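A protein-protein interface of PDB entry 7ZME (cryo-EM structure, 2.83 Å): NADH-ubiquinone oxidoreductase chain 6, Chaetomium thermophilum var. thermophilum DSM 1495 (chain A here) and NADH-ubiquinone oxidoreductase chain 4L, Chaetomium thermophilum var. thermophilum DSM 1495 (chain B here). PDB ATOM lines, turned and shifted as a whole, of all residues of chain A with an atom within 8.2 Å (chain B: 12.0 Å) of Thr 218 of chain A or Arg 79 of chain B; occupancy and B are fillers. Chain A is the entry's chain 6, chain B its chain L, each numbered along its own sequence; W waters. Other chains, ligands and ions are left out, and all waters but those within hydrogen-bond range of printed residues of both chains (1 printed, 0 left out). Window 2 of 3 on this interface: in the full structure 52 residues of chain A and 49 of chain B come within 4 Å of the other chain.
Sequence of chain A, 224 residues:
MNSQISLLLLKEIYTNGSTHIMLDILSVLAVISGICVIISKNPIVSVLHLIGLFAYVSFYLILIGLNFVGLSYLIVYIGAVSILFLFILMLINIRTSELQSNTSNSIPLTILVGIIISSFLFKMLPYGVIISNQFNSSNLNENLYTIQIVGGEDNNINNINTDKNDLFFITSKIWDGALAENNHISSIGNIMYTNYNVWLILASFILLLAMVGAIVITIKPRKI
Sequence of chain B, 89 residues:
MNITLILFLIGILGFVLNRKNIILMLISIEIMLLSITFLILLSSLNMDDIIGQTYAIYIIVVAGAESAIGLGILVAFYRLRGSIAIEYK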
ATOM      1  N   PHE A  87      -5.957 -10.233   5.133  1.00  0.00           N
ATOM      2  CA  PHE A  87      -6.321 -10.323   6.574  1.00  0.00           C
ATOM      3  C   PHE A  87      -6.031 -11.729   7.106  1.00  0.00           C
ATOM      4  O   PHE A  87      -5.699 -11.846   8.282  1.00  0.00           O
ATOM      5  CB  PHE A  87      -7.750  -9.822   6.795  1.00  0.00           C
ATOM      6  CG  PHE A  87      -7.891  -8.330   6.947  1.00  0.00           C
ATOM      7  CD1 PHE A  87      -7.657  -7.478   5.882  1.00  0.00           C
ATOM      8  CD2 PHE A  87      -8.281  -7.775   8.154  1.00  0.00           C
ATOM      9  CE1 PHE A  87      -7.795  -6.108   6.022  1.00  0.00           C
ATOM     10  CE2 PHE A  87      -8.422  -6.405   8.291  1.00  0.00           C
ATOM     11  CZ  PHE A  87      -8.177  -5.574   7.227  1.00  0.00           C
ATOM     12  N   MET A  90      -2.623 -11.891   8.362  1.00  0.00           N
ATOM     13  CA  MET A  90      -2.394 -11.092   9.557  1.00  0.00           C
ATOM     14  C   MET A  90      -3.037 -11.680  10.806  1.00  0.00           C
ATOM     15  O   MET A  90      -2.470 -11.556  11.896  1.00  0.00           O
ATOM     16  CB  MET A  90      -2.899  -9.667   9.309  1.00  0.00           C
ATOM     17  CG  MET A  90      -2.689  -8.688  10.438  1.00  0.00           C
ATOM     18  SD  MET A  90      -3.300  -7.054   9.985  1.00  0.00           S
ATOM     19  CE  MET A  90      -5.065  -7.313  10.016  1.00  0.00           C
ATOM     20  N   LEU A  91      -4.172 -12.370  10.655  1.00  0.00           N
ATOM     21  CA  LEU A  91      -4.925 -12.831  11.852  1.00  0.00           C
ATOM     22  C   LEU A  91      -5.000 -14.360  11.954  1.00  0.00           C
ATOM     23  O   LEU A  91      -5.632 -14.830  12.908  1.00  0.00           O
ATOM     24  CB  LEU A  91      -6.334 -12.229  11.813  1.00  0.00           C
ATOM     25  CG  LEU A  91      -6.452 -10.755  11.429  1.00  0.00           C
ATOM     26  CD1 LEU A  91      -7.894 -10.399  11.109  1.00  0.00           C
ATOM     27  CD2 LEU A  91      -5.919  -9.857  12.528  1.00  0.00           C
ATOM     28  N   MET A 211     -16.869   3.656   6.635  1.00  0.00           N
ATOM     29  CA  MET A 211     -15.570   4.370   6.519  1.00  0.00           C
ATOM     30  C   MET A 211     -15.157   4.934   7.878  1.00  0.00           C
ATOM     31  O   MET A 211     -13.968   4.860   8.201  1.00  0.00           O
ATOM     32  CB  MET A 211     -15.669   5.514   5.508  1.00  0.00           C
ATOM     33  CG  MET A 211     -16.054   5.084   4.115  1.00  0.00           C
ATOM     34  SD  MET A 211     -16.008   6.497   2.987  1.00  0.00           S
ATOM     35  CE  MET A 211     -14.287   6.969   3.136  1.00  0.00           C
ATOM     36  N   VAL A 212     -16.107   5.473   8.639  1.00  0.00           N
ATOM     37  CA  VAL A 212     -15.801   6.107   9.955  1.00  0.00           C
ATOM     38  C   VAL A 212     -15.643   5.024  11.022  1.00  0.00           C
ATOM     39  O   VAL A 212     -14.674   5.104  11.785  1.00  0.00           O
ATOM     40  CB  VAL A 212     -16.883   7.139  10.334  1.00  0.00           C
ATOM     41  CG1 VAL A 212     -16.746   7.628  11.769  1.00  0.00           C
ATOM     42  CG2 VAL A 212     -16.907   8.306   9.363  1.00  0.00           C
ATOM     43  N   GLY A 213     -16.536   4.037  11.039  1.00  0.00           N
ATOM     44  CA  GLY A 213     -16.512   2.987  12.072  1.00  0.00           C
ATOM     45  C   GLY A 213     -15.352   2.029  11.948  1.00  0.00           C
ATOM     46  O   GLY A 213     -14.779   1.683  12.985  1.00  0.00           O
ATOM     47  N   ALA A 214     -15.041   1.571  10.737  1.00  0.00           N
ATOM     48  CA  ALA A 214     -13.970   0.558  10.608  1.00  0.00           C
ATOM     49  C   ALA A 214     -12.659   1.195  11.067  1.00  0.00           C
ATOM     50  O   ALA A 214     -11.881   0.514  11.739  1.00  0.00           O
ATOM     51  CB  ALA A 214     -13.893   0.006   9.203  1.00  0.00           C
ATOM     52  N   ILE A 215     -12.444   2.455  10.704  1.00  0.00           N
ATOM     53  CA  ILE A 215     -11.233   3.199  11.150  1.00  0.00           C
ATOM     54  C   ILE A 215     -11.272   3.445  12.659  1.00  0.00           C
ATOM     55  O   ILE A 215     -10.246   3.229  13.295  1.00  0.00           O
ATOM     56  CB  ILE A 215     -11.056   4.495  10.331  1.00  0.00           C
ATOM     57  CG1 ILE A 215     -10.277   4.226   9.043  1.00  0.00           C
ATOM     58  CG2 ILE A 215     -10.379   5.579  11.156  1.00  0.00           C
ATOM     59  CD1 ILE A 215     -10.820   3.098   8.193  1.00  0.00           C
ATOM     60  N   VAL A 216     -12.428   3.810  13.217  1.00  0.00           N
ATOM     61  CA  VAL A 216     -12.490   4.177  14.663  1.00  0.00           C
ATOM     62  C   VAL A 216     -12.080   2.978  15.523  1.00  0.00           C
ATOM     63  O   VAL A 216     -11.371   3.201  16.516  1.00  0.00           O
ATOM     64  CB  VAL A 216     -13.836   4.805  15.092  1.00  0.00           C
ATOM     65  CG1 VAL A 216     -14.954   3.791  15.247  1.00  0.00           C
ATOM     66  CG2 VAL A 216     -13.687   5.580  16.387  1.00  0.00           C
ATOM     67  N   ILE A 217     -12.479   1.763  15.146  1.00  0.00           N
ATOM     68  CA  ILE A 217     -12.216   0.576  16.009  1.00  0.00           C
ATOM     69  C   ILE A 217     -10.817   0.010  15.789  1.00  0.00           C
ATOM     70  O   ILE A 217     -10.419  -0.834  16.590  1.00  0.00           O
ATOM     71  CB  ILE A 217     -13.302  -0.495  15.816  1.00  0.00           C
ATOM     72  CG1 ILE A 217     -13.397  -0.956  14.361  1.00  0.00           C
ATOM     73  CG2 ILE A 217     -14.640   0.002  16.341  1.00  0.00           C
ATOM     74  CD1 ILE A 217     -14.623  -1.777  14.066  1.00  0.00           C
ATOM     75  N   THR A 218     -10.119   0.424  14.733  1.00  0.00           N
ATOM     76  CA  THR A 218      -8.806  -0.184  14.413  1.00  0.00           C
ATOM     77  C   THR A 218      -7.691   0.860  14.388  1.00  0.00           C
ATOM     78  O   THR A 218      -6.534   0.449  14.232  1.00  0.00           O
ATOM     79  CB  THR A 218      -8.868  -0.894  13.057  1.00  0.00           C
ATOM     80  OG1 THR A 218      -9.118   0.088  12.053  1.00  0.00           O
ATOM     81  CG2 THR A 218      -9.916  -1.983  12.994  1.00  0.00           C
ATOM     82  N   ILE A 219      -8.013   2.145  14.529  1.00  0.00           N
ATOM     83  CA  ILE A 219      -6.977   3.209  14.381  1.00  0.00           C
ATOM     84  C   ILE A 219      -5.929   3.105  15.488  1.00  0.00           C
ATOM     85  O   ILE A 219      -6.294   2.873  16.636  1.00  0.00           O
ATOM     86  CB  ILE A 219      -7.609   4.617  14.285  1.00  0.00           C
ATOM     87  CG1 ILE A 219      -6.597   5.678  13.844  1.00  0.00           C
ATOM     88  CG2 ILE A 219      -8.318   5.013  15.569  1.00  0.00           C
ATOM     89  CD1 ILE A 219      -5.938   5.375  12.524  1.00  0.00           C
ATOM     90  N   LYS A 220      -4.662   3.316  15.156  1.00  0.00           N
ATOM     91  CA  LYS A 220      -3.626   3.341  16.214  1.00  0.00           C
ATOM     92  C   LYS A 220      -3.780   4.637  17.035  1.00  0.00           C
ATOM     93  O   LYS A 220      -4.004   5.683  16.402  1.00  0.00           O
ATOM     94  CB  LYS A 220      -2.225   3.223  15.604  1.00  0.00           C
ATOM     95  CG  LYS A 220      -1.909   1.877  14.966  1.00  0.00           C
ATOM     96  CD  LYS A 220      -0.514   1.806  14.383  1.00  0.00           C
ATOM     97  CE  LYS A 220      -0.167   0.435  13.845  1.00  0.00           C
ATOM     98  NZ  LYS A 220      -0.214  -0.599  14.906  1.00  0.00           N
ATOM     99  N   PRO A 221      -3.675   4.655  18.390  1.00  0.00           N
ATOM    100  CA  PRO A 221      -3.869   5.903  19.139  1.00  0.00           C
ATOM    101  C   PRO A 221      -2.778   6.916  18.834  1.00  0.00           C
ATOM    102  O   PRO A 221      -1.635   6.559  18.540  1.00  0.00           O
ATOM    103  CB  PRO A 221      -3.821   5.450  20.602  1.00  0.00           C
ATOM    104  CG  PRO A 221      -3.011   4.198  20.577  1.00  0.00           C
ATOM    105  CD  PRO A 221      -3.329   3.526  19.272  1.00  0.00           C
ATOM    106  N   ILE B  22     -13.169 -17.348  12.168  1.00  0.00           N
ATOM    107  CA  ILE B  22     -14.273 -16.368  11.991  1.00  0.00           C
ATOM    108  C   ILE B  22     -14.149 -15.697  10.616  1.00  0.00           C
ATOM    109  O   ILE B  22     -15.165 -15.176  10.128  1.00  0.00           O
ATOM    110  CB  ILE B  22     -14.235 -15.373  13.167  1.00  0.00           C
ATOM    111  CG1 ILE B  22     -14.160 -16.104  14.508  1.00  0.00           C
ATOM    112  CG2 ILE B  22     -15.397 -14.396  13.119  1.00  0.00           C
ATOM    113  CD1 ILE B  22     -13.566 -15.280  15.621  1.00  0.00           C
ATOM    114  N   ILE B  23     -12.964 -15.694  10.006  1.00  0.00           N
ATOM    115  CA  ILE B  23     -12.852 -15.155   8.615  1.00  0.00           C
ATOM    116  C   ILE B  23     -13.674 -16.021   7.647  1.00  0.00           C
ATOM    117  O   ILE B  23     -14.338 -15.445   6.780  1.00  0.00           O
ATOM    118  CB  ILE B  23     -11.383 -14.939   8.184  1.00  0.00           C
ATOM    119  CG1 ILE B  23     -10.813 -13.653   8.784  1.00  0.00           C
ATOM    120  CG2 ILE B  23     -11.251 -14.924   6.671  1.00  0.00           C
ATOM    121  CD1 ILE B  23      -9.489 -13.228   8.198  1.00  0.00           C
ATOM    122  N   LEU B  26     -17.275 -15.047   7.936  1.00  0.00           N
ATOM    123  CA  LEU B  26     -17.532 -13.798   7.169  1.00  0.00           C
ATOM    124  C   LEU B  26     -17.566 -14.092   5.660  1.00  0.00           C
ATOM    125  O   LEU B  26     -18.277 -13.368   4.949  1.00  0.00           O
ATOM    126  CB  LEU B  26     -16.406 -12.824   7.533  1.00  0.00           C
ATOM    127  CG  LEU B  26     -16.527 -11.397   7.009  1.00  0.00           C
ATOM    128  CD1 LEU B  26     -17.797 -10.733   7.515  1.00  0.00           C
ATOM    129  CD2 LEU B  26     -15.311 -10.583   7.413  1.00  0.00           C
ATOM    130  N   ALA B  65     -19.642  -3.221   2.517  1.00  0.00           N
ATOM    131  CA  ALA B  65     -19.645  -2.448   3.754  1.00  0.00           C
ATOM    132  C   ALA B  65     -19.697  -3.363   4.969  1.00  0.00           C
ATOM    133  O   ALA B  65     -19.048  -3.097   5.986  1.00  0.00           O
ATOM    134  CB  ALA B  65     -20.819  -1.471   3.760  1.00  0.00           C
ATOM    135  N   GLU B  66     -20.471  -4.445   4.882  1.00  0.00           N
ATOM    136  CA  GLU B  66     -20.524  -5.411   5.973  1.00  0.00           C
ATOM    137  C   GLU B  66     -19.192  -6.130   6.141  1.00  0.00           C
ATOM    138  O   GLU B  66     -18.777  -6.423   7.268  1.00  0.00           O
ATOM    139  CB  GLU B  66     -21.655  -6.409   5.728  1.00  0.00           C
ATOM    140  CG  GLU B  66     -21.609  -7.640   6.612  1.00  0.00           C
ATOM    141  CD  GLU B  66     -22.793  -8.555   6.393  1.00  0.00           C
ATOM    142  OE1 GLU B  66     -23.552  -8.322   5.430  1.00  0.00           O
ATOM    143  OE2 GLU B  66     -22.968  -9.504   7.185  1.00  0.00           O
ATOM    144  N   SER B  67     -18.506  -6.418   5.036  1.00  0.00           N
ATOM    145  CA  SER B  67     -17.225  -7.110   5.128  1.00  0.00           C
ATOM    146  C   SER B  67     -16.127  -6.199   5.660  1.00  0.00           C
ATOM    147  O   SER B  67     -15.144  -6.685   6.225  1.00  0.00           O
ATOM    148  CB  SER B  67     -16.842  -7.686   3.765  1.00  0.00           C
ATOM    149  OG  SER B  67     -16.570  -6.662   2.829  1.00  0.00           O
ATOM    150  N   ALA B  68     -16.273  -4.884   5.494  1.00  0.00           N
ATOM    151  CA  ALA B  68     -15.327  -3.951   6.096  1.00  0.00           C
ATOM    152  C   ALA B  68     -15.537  -3.835   7.600  1.00  0.00           C
ATOM    153  O   ALA B  68     -14.566  -3.802   8.364  1.00  0.00           O
ATOM    154  CB  ALA B  68     -15.446  -2.580   5.434  1.00  0.00           C
ATOM    155  N   ILE B  69     -16.793  -3.764   8.043  1.00  0.00           N
ATOM    156  CA  ILE B  69     -17.078  -3.722   9.473  1.00  0.00           C
ATOM    157  C   ILE B  69     -16.707  -5.044  10.128  1.00  0.00           C
ATOM    158  O   ILE B  69     -16.223  -5.074  11.265  1.00  0.00           O
ATOM    159  CB  ILE B  69     -18.555  -3.355   9.711  1.00  0.00           C
ATOM    160  CG1 ILE B  69     -18.879  -2.026   9.042  1.00  0.00           C
ATOM    161  CG2 ILE B  69     -18.869  -3.284  11.196  1.00  0.00           C
ATOM    162  CD1 ILE B  69     -18.100  -0.875   9.605  1.00  0.00           C
ATOM    163  N   GLY B  70     -16.921  -6.155   9.425  1.00  0.00           N
ATOM    164  CA  GLY B  70     -16.522  -7.444   9.963  1.00  0.00           C
ATOM    165  C   GLY B  70     -15.020  -7.592  10.093  1.00  0.00           C
ATOM    166  O   GLY B  70     -14.525  -8.089  11.106  1.00  0.00           O
ATOM    167  N   LEU B  71     -14.275  -7.175   9.070  1.00  0.00           N
ATOM    168  CA  LEU B  71     -12.822  -7.255   9.147  1.00  0.00           C
ATOM    169  C   LEU B  71     -12.277  -6.283  10.182  1.00  0.00           C
ATOM    170  O   LEU B  71     -11.292  -6.581  10.864  1.00  0.00           O
ATOM    171  CB  LEU B  71     -12.205  -6.993   7.773  1.00  0.00           C
ATOM    172  CG  LEU B  71     -12.218  -8.181   6.808  1.00  0.00           C
ATOM    173  CD1 LEU B  71     -11.522  -7.833   5.516  1.00  0.00           C
ATOM    174  CD2 LEU B  71     -11.586  -9.404   7.447  1.00  0.00           C
ATOM    175  N   GLY B  72     -12.906  -5.114  10.310  1.00  0.00           N
ATOM    176  CA  GLY B  72     -12.488  -4.167  11.329  1.00  0.00           C
ATOM    177  C   GLY B  72     -12.758  -4.656  12.738  1.00  0.00           C
ATOM    178  O   GLY B  72     -11.963  -4.414  13.649  1.00  0.00           O
ATOM    179  N   ILE B  73     -13.884  -5.343  12.940  1.00  0.00           N
ATOM    180  CA  ILE B  73     -14.196  -5.870  14.262  1.00  0.00           C
ATOM    181  C   ILE B  73     -13.317  -7.074  14.578  1.00  0.00           C
ATOM    182  O   ILE B  73     -12.937  -7.285  15.735  1.00  0.00           O
ATOM    183  CB  ILE B  73     -15.699  -6.196  14.371  1.00  0.00           C
ATOM    184  CG1 ILE B  73     -16.506  -4.901  14.476  1.00  0.00           C
ATOM    185  CG2 ILE B  73     -15.988  -7.066  15.579  1.00  0.00           C
ATOM    186  CD1 ILE B  73     -17.989  -5.081  14.320  1.00  0.00           C
ATOM    187  N   LEU B  74     -12.969  -7.873  13.564  1.00  0.00           N
ATOM    188  CA  LEU B  74     -12.023  -8.966  13.780  1.00  0.00           C
ATOM    189  C   LEU B  74     -10.672  -8.455  14.252  1.00  0.00           C
ATOM    190  O   LEU B  74     -10.063  -9.044  15.151  1.00  0.00           O
ATOM    191  CB  LEU B  74     -11.843  -9.789  12.509  1.00  0.00           C
ATOM    192  CG  LEU B  74     -12.930 -10.792  12.183  1.00  0.00           C
ATOM    193  CD1 LEU B  74     -12.658 -11.421  10.841  1.00  0.00           C
ATOM    194  CD2 LEU B  74     -12.899 -11.835  13.274  1.00  0.00           C
ATOM    195  N   VAL B  75     -10.176  -7.378  13.647  1.00  0.00           N
ATOM    196  CA  VAL B  75      -8.884  -6.837  14.054  1.00  0.00           C
ATOM    197  C   VAL B  75      -8.931  -6.420  15.518  1.00  0.00           C
ATOM    198  O   VAL B  75      -8.040  -6.754  16.305  1.00  0.00           O
ATOM    199  CB  VAL B  75      -8.480  -5.670  13.137  1.00  0.00           C
ATOM    200  CG1 VAL B  75      -7.359  -4.865  13.759  1.00  0.00           C
ATOM    201  CG2 VAL B  75      -8.061  -6.195  11.793  1.00  0.00           C
ATOM    202  N   ALA B  76     -10.020  -5.767  15.921  1.00  0.00           N
ATOM    203  CA  ALA B  76     -10.214  -5.384  17.335  1.00  0.00           C
ATOM    204  C   ALA B  76     -10.179  -6.620  18.236  1.00  0.00           C
ATOM    205  O   ALA B  76      -9.458  -6.593  19.240  1.00  0.00           O
ATOM    206  CB  ALA B  76     -11.521  -4.650  17.440  1.00  0.00           C
ATOM    207  N   PHE B  77     -10.956  -7.643  17.902  1.00  0.00           N
ATOM    208  CA  PHE B  77     -11.028  -8.903  18.680  1.00  0.00           C
ATOM    209  C   PHE B  77      -9.676  -9.618  18.719  1.00  0.00           C
ATOM    210  O   PHE B  77      -9.293 -10.019  19.818  1.00  0.00           O
ATOM    211  CB  PHE B  77     -12.108  -9.778  18.034  1.00  0.00           C
ATOM    212  CG  PHE B  77     -12.333 -11.147  18.617  1.00  0.00           C
ATOM    213  CD1 PHE B  77     -13.142 -11.318  19.727  1.00  0.00           C
ATOM    214  CD2 PHE B  77     -11.782 -12.269  18.022  1.00  0.00           C
ATOM    215  CE1 PHE B  77     -13.367 -12.581  20.249  1.00  0.00           C
ATOM    216  CE2 PHE B  77     -12.008 -13.531  18.546  1.00  0.00           C
ATOM    217  CZ  PHE B  77     -12.802 -13.684  19.654  1.00  0.00           C
ATOM    218  N   TYR B  78      -8.984  -9.754  17.583  1.00  0.00           N
ATOM    219  CA  TYR B  78      -7.675 -10.457  17.509  1.00  0.00           C
ATOM    220  C   TYR B  78      -6.634  -9.710  18.342  1.00  0.00           C
ATOM    221  O   TYR B  78      -5.792 -10.345  18.957  1.00  0.00           O
ATOM    222  CB  TYR B  78      -7.251 -10.640  16.052  1.00  0.00           C
ATOM    223  CG  TYR B  78      -5.936 -11.345  15.844  1.00  0.00           C
ATOM    224  CD1 TYR B  78      -5.873 -12.724  15.792  1.00  0.00           C
ATOM    225  CD2 TYR B  78      -4.758 -10.635  15.693  1.00  0.00           C
ATOM    226  CE1 TYR B  78      -4.672 -13.383  15.598  1.00  0.00           C
ATOM    227  CE2 TYR B  78      -3.549 -11.277  15.499  1.00  0.00           C
ATOM    228  CZ  TYR B  78      -3.508 -12.657  15.451  1.00  0.00           C
ATOM    229  OH  TYR B  78      -2.323 -13.301  15.260  1.00  0.00           O
ATOM    230  N   ARG B  79      -6.696  -8.387  18.354  1.00  0.00           N
ATOM    231  CA  ARG B  79      -5.686  -7.575  19.062  1.00  0.00           C
ATOM    232  C   ARG B  79      -5.700  -7.971  20.527  1.00  0.00           C
ATOM    233  O   ARG B  79      -4.635  -7.946  21.158  1.00  0.00           O
ATOM    234  CB  ARG B  79      -5.951  -6.086  18.847  1.00  0.00           C
ATOM    235  CG  ARG B  79      -5.319  -5.539  17.579  1.00  0.00           C
ATOM    236  CD  ARG B  79      -5.682  -4.097  17.308  1.00  0.00           C
ATOM    237  NE  ARG B  79      -5.004  -3.631  16.109  1.00  0.00           N
ATOM    238  CZ  ARG B  79      -5.096  -2.398  15.635  1.00  0.00           C
ATOM    239  NH1 ARG B  79      -4.438  -2.062  14.540  1.00  0.00           N
ATOM    240  NH2 ARG B  79      -5.837  -1.502  16.261  1.00  0.00           N
ATOM    241  N   LEU B  80      -6.878  -8.290  21.045  1.00  0.00           N
ATOM    242  CA  LEU B  80      -6.984  -8.659  22.465  1.00  0.00           C
ATOM    243  C   LEU B  80      -6.914 -10.184  22.659  1.00  0.00           C
ATOM    244  O   LEU B  80      -6.092 -10.625  23.469  1.00  0.00           O
ATOM    245  CB  LEU B  80      -8.278  -8.023  22.962  1.00  0.00           C
ATOM    246  CG  LEU B  80      -8.345  -6.508  22.777  1.00  0.00           C
ATOM    247  CD1 LEU B  80      -9.753  -5.987  22.976  1.00  0.00           C
ATOM    248  CD2 LEU B  80      -7.379  -5.798  23.709  1.00  0.00           C
ATOM    249  N   ARG B  81      -7.719 -10.959  21.939  1.00  0.00           N
ATOM    250  CA  ARG B  81      -7.752 -12.435  22.079  1.00  0.00           C
ATOM    251  C   ARG B  81      -6.485 -13.102  21.538  1.00  0.00           C
ATOM    252  O   ARG B  81      -6.043 -14.087  22.154  1.00  0.00           O
ATOM    253  CB  ARG B  81      -9.034 -13.010  21.468  1.00  0.00           C
ATOM    254  CG  ARG B  81      -9.231 -14.485  21.778  1.00  0.00           C
ATOM    255  CD  ARG B  81     -10.673 -14.818  22.096  1.00  0.00           C
ATOM    256  NE  ARG B  81     -11.280 -13.821  22.964  1.00  0.00           N
ATOM    257  CZ  ARG B  81     -11.344 -13.914  24.286  1.00  0.00           C
ATOM    258  NH1 ARG B  81     -10.834 -14.966  24.901  1.00  0.00           N
ATOM    259  NH2 ARG B  81     -11.916 -12.953  24.989  1.00  0.00           N
ATOM    260  N   GLY B  82      -5.969 -12.640  20.399  1.00  0.00           N
ATOM    261  CA  GLY B  82      -4.747 -13.209  19.794  1.00  0.00           C
ATOM    262  C   GLY B  82      -5.007 -14.435  18.939  1.00  0.00           C
ATOM    263  O   GLY B  82      -4.038 -14.990  18.405  1.00  0.00           O
ATOM    264  N   SER B  83      -6.254 -14.869  18.829  1.00  0.00           N
ATOM    265  CA  SER B  83      -6.608 -15.990  17.930  1.00  0.00           C
ATOM    266  C   SER B  83      -8.003 -15.711  17.390  1.00  0.00           C
ATOM    267  O   SER B  83      -8.800 -15.123  18.141  1.00  0.00           O
ATOM    268  CB  SER B  83      -6.597 -17.289  18.682  1.00  0.00           C
ATOM    269  OG  SER B  83      -7.256 -18.309  17.955  1.00  0.00           O
ATOM    270  N   ILE B  84      -8.252 -15.945  16.102  1.00  0.00           N
ATOM    271  CA  ILE B  84      -9.641 -15.782  15.582  1.00  0.00           C
ATOM    272  C   ILE B  84     -10.087 -17.163  15.135  1.00  0.00           C
ATOM    273  O   ILE B  84     -10.874 -17.266  14.189  1.00  0.00           O
ATOM    274  CB  ILE B  84      -9.754 -14.726  14.468  1.00  0.00           C
ATOM    275  CG1 ILE B  84      -8.902 -15.066  13.244  1.00  0.00           C
ATOM    276  CG2 ILE B  84      -9.455 -13.333  14.997  1.00  0.00           C
ATOM    277  CD1 ILE B  84      -9.592 -14.777  11.938  1.00  0.00           C
ATOM    278  N   ALA B  85      -9.616 -18.178  15.847  1.00  0.00           N
ATOM    279  CA  ALA B  85      -9.952 -19.565  15.491  1.00  0.00           C
ATOM    280  C   ALA B  85     -11.103 -20.004  16.387  1.00  0.00           C
ATOM    281  O   ALA B  85     -10.934 -19.968  17.619  1.00  0.00           O
ATOM    282  CB  ALA B  85      -8.739 -20.406  15.741  1.00  0.00           C
HETATM  283  O   HOH W   1      -8.689  -2.177  17.890  1.00  0.00           O
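Of the 14 printed residues of chain A, 6 touch a printed residue of chain B.
Along chain A the printed residues that touch a printed residue of chain B span positions 87 to 218.
Among the printed residues, no Asp or Glu carboxylate lies within 4 Å of a Lys or Arg side-chain nitrogen of the other chain.
The guanidinium group (NH2) of Arg 79 of chain B sits at hydrogen-bond distance from the backbone carbonyl oxygen (O) of Thr 218 of chain A, at 2.9 Å.
Of the printed residues of chain B, Leu 91 of chain A touches Tyr 78 and Ile 84.
Of chain B, only Ala 68 comes within 4 Å of Ala 214 of chain A.
No residue of chain B comes within 4 Å of Ile 215 of chain A.
No residue of chain B comes within 4 Å of Val 216 of chain A.
Ile 217 of chain A touches just these residues of chain B: Gly 72 (3.7 Å) and Ile 73 (3.7 Å).
No residue of chain B comes within 4 Å of Ile 219 of chain A.
No residue of chain B comes within 4 Å of Lys 220 of chain A.
Ile 22 of chain B touches none of the printed residues of chain A.
Of the printed residues of chain A, Ile 23 of chain B touches Phe 87.
Printed residues of chain A within 4 Å of Val 75 of chain B: Phe 87, Met 90 and Thr 218.
Of chain A, only Thr 218 comes within 4 Å of Arg 79 of chain B.
Of the printed residues of chain A, Ile 84 of chain B touches Leu 91 (3.3 Å).
The nearest residue of chain B that does not touch Thr 218 of chain A is Ala 76 of chain B (4.8 Å).
The nearest printed residue of chain B that does not touch Met 90 of chain A is Leu 71 of chain B (6.3 Å).
The backbone carbonyl oxygen (O) of Ile 84 of chain B lies within hydrogen-bond range of the backbone NH (N) of Ile 22 of chain B (3.1 Å).
O of Ala 214 of chain A is in hydrogen-bond range of OG1 of Thr 218 of chain A.
Water W1 bridges O of Ile 217 of chain A (2.5 Å) and NH2 of Arg 79 of chain B (3.4 Å).
Among the printed residues, merely in contact across the chains: Phe 87 of chain A with Ile 23 of chain B, Phe 87 of chain A with Leu 71 of chain B, Phe 87 of chain A with Val 75 of chain B, Met 90 of chain A with Val 75 of chain B, Met 90 of chain A with Tyr 78 of chain B, Leu 91 of chain A with Tyr 78 of chain B, Leu 91 of chain A with Ile 84 of chain B, Ala 214 of chain A with Ala 68 of chain B, Ile 217 of chain A with Gly 72 of chain B, Ile 217 of chain A with Ile 73 of chain B, Thr 218 of chain A with Gly 72 of chain B and Thr 218 of chain A with Val 75 of chain B.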
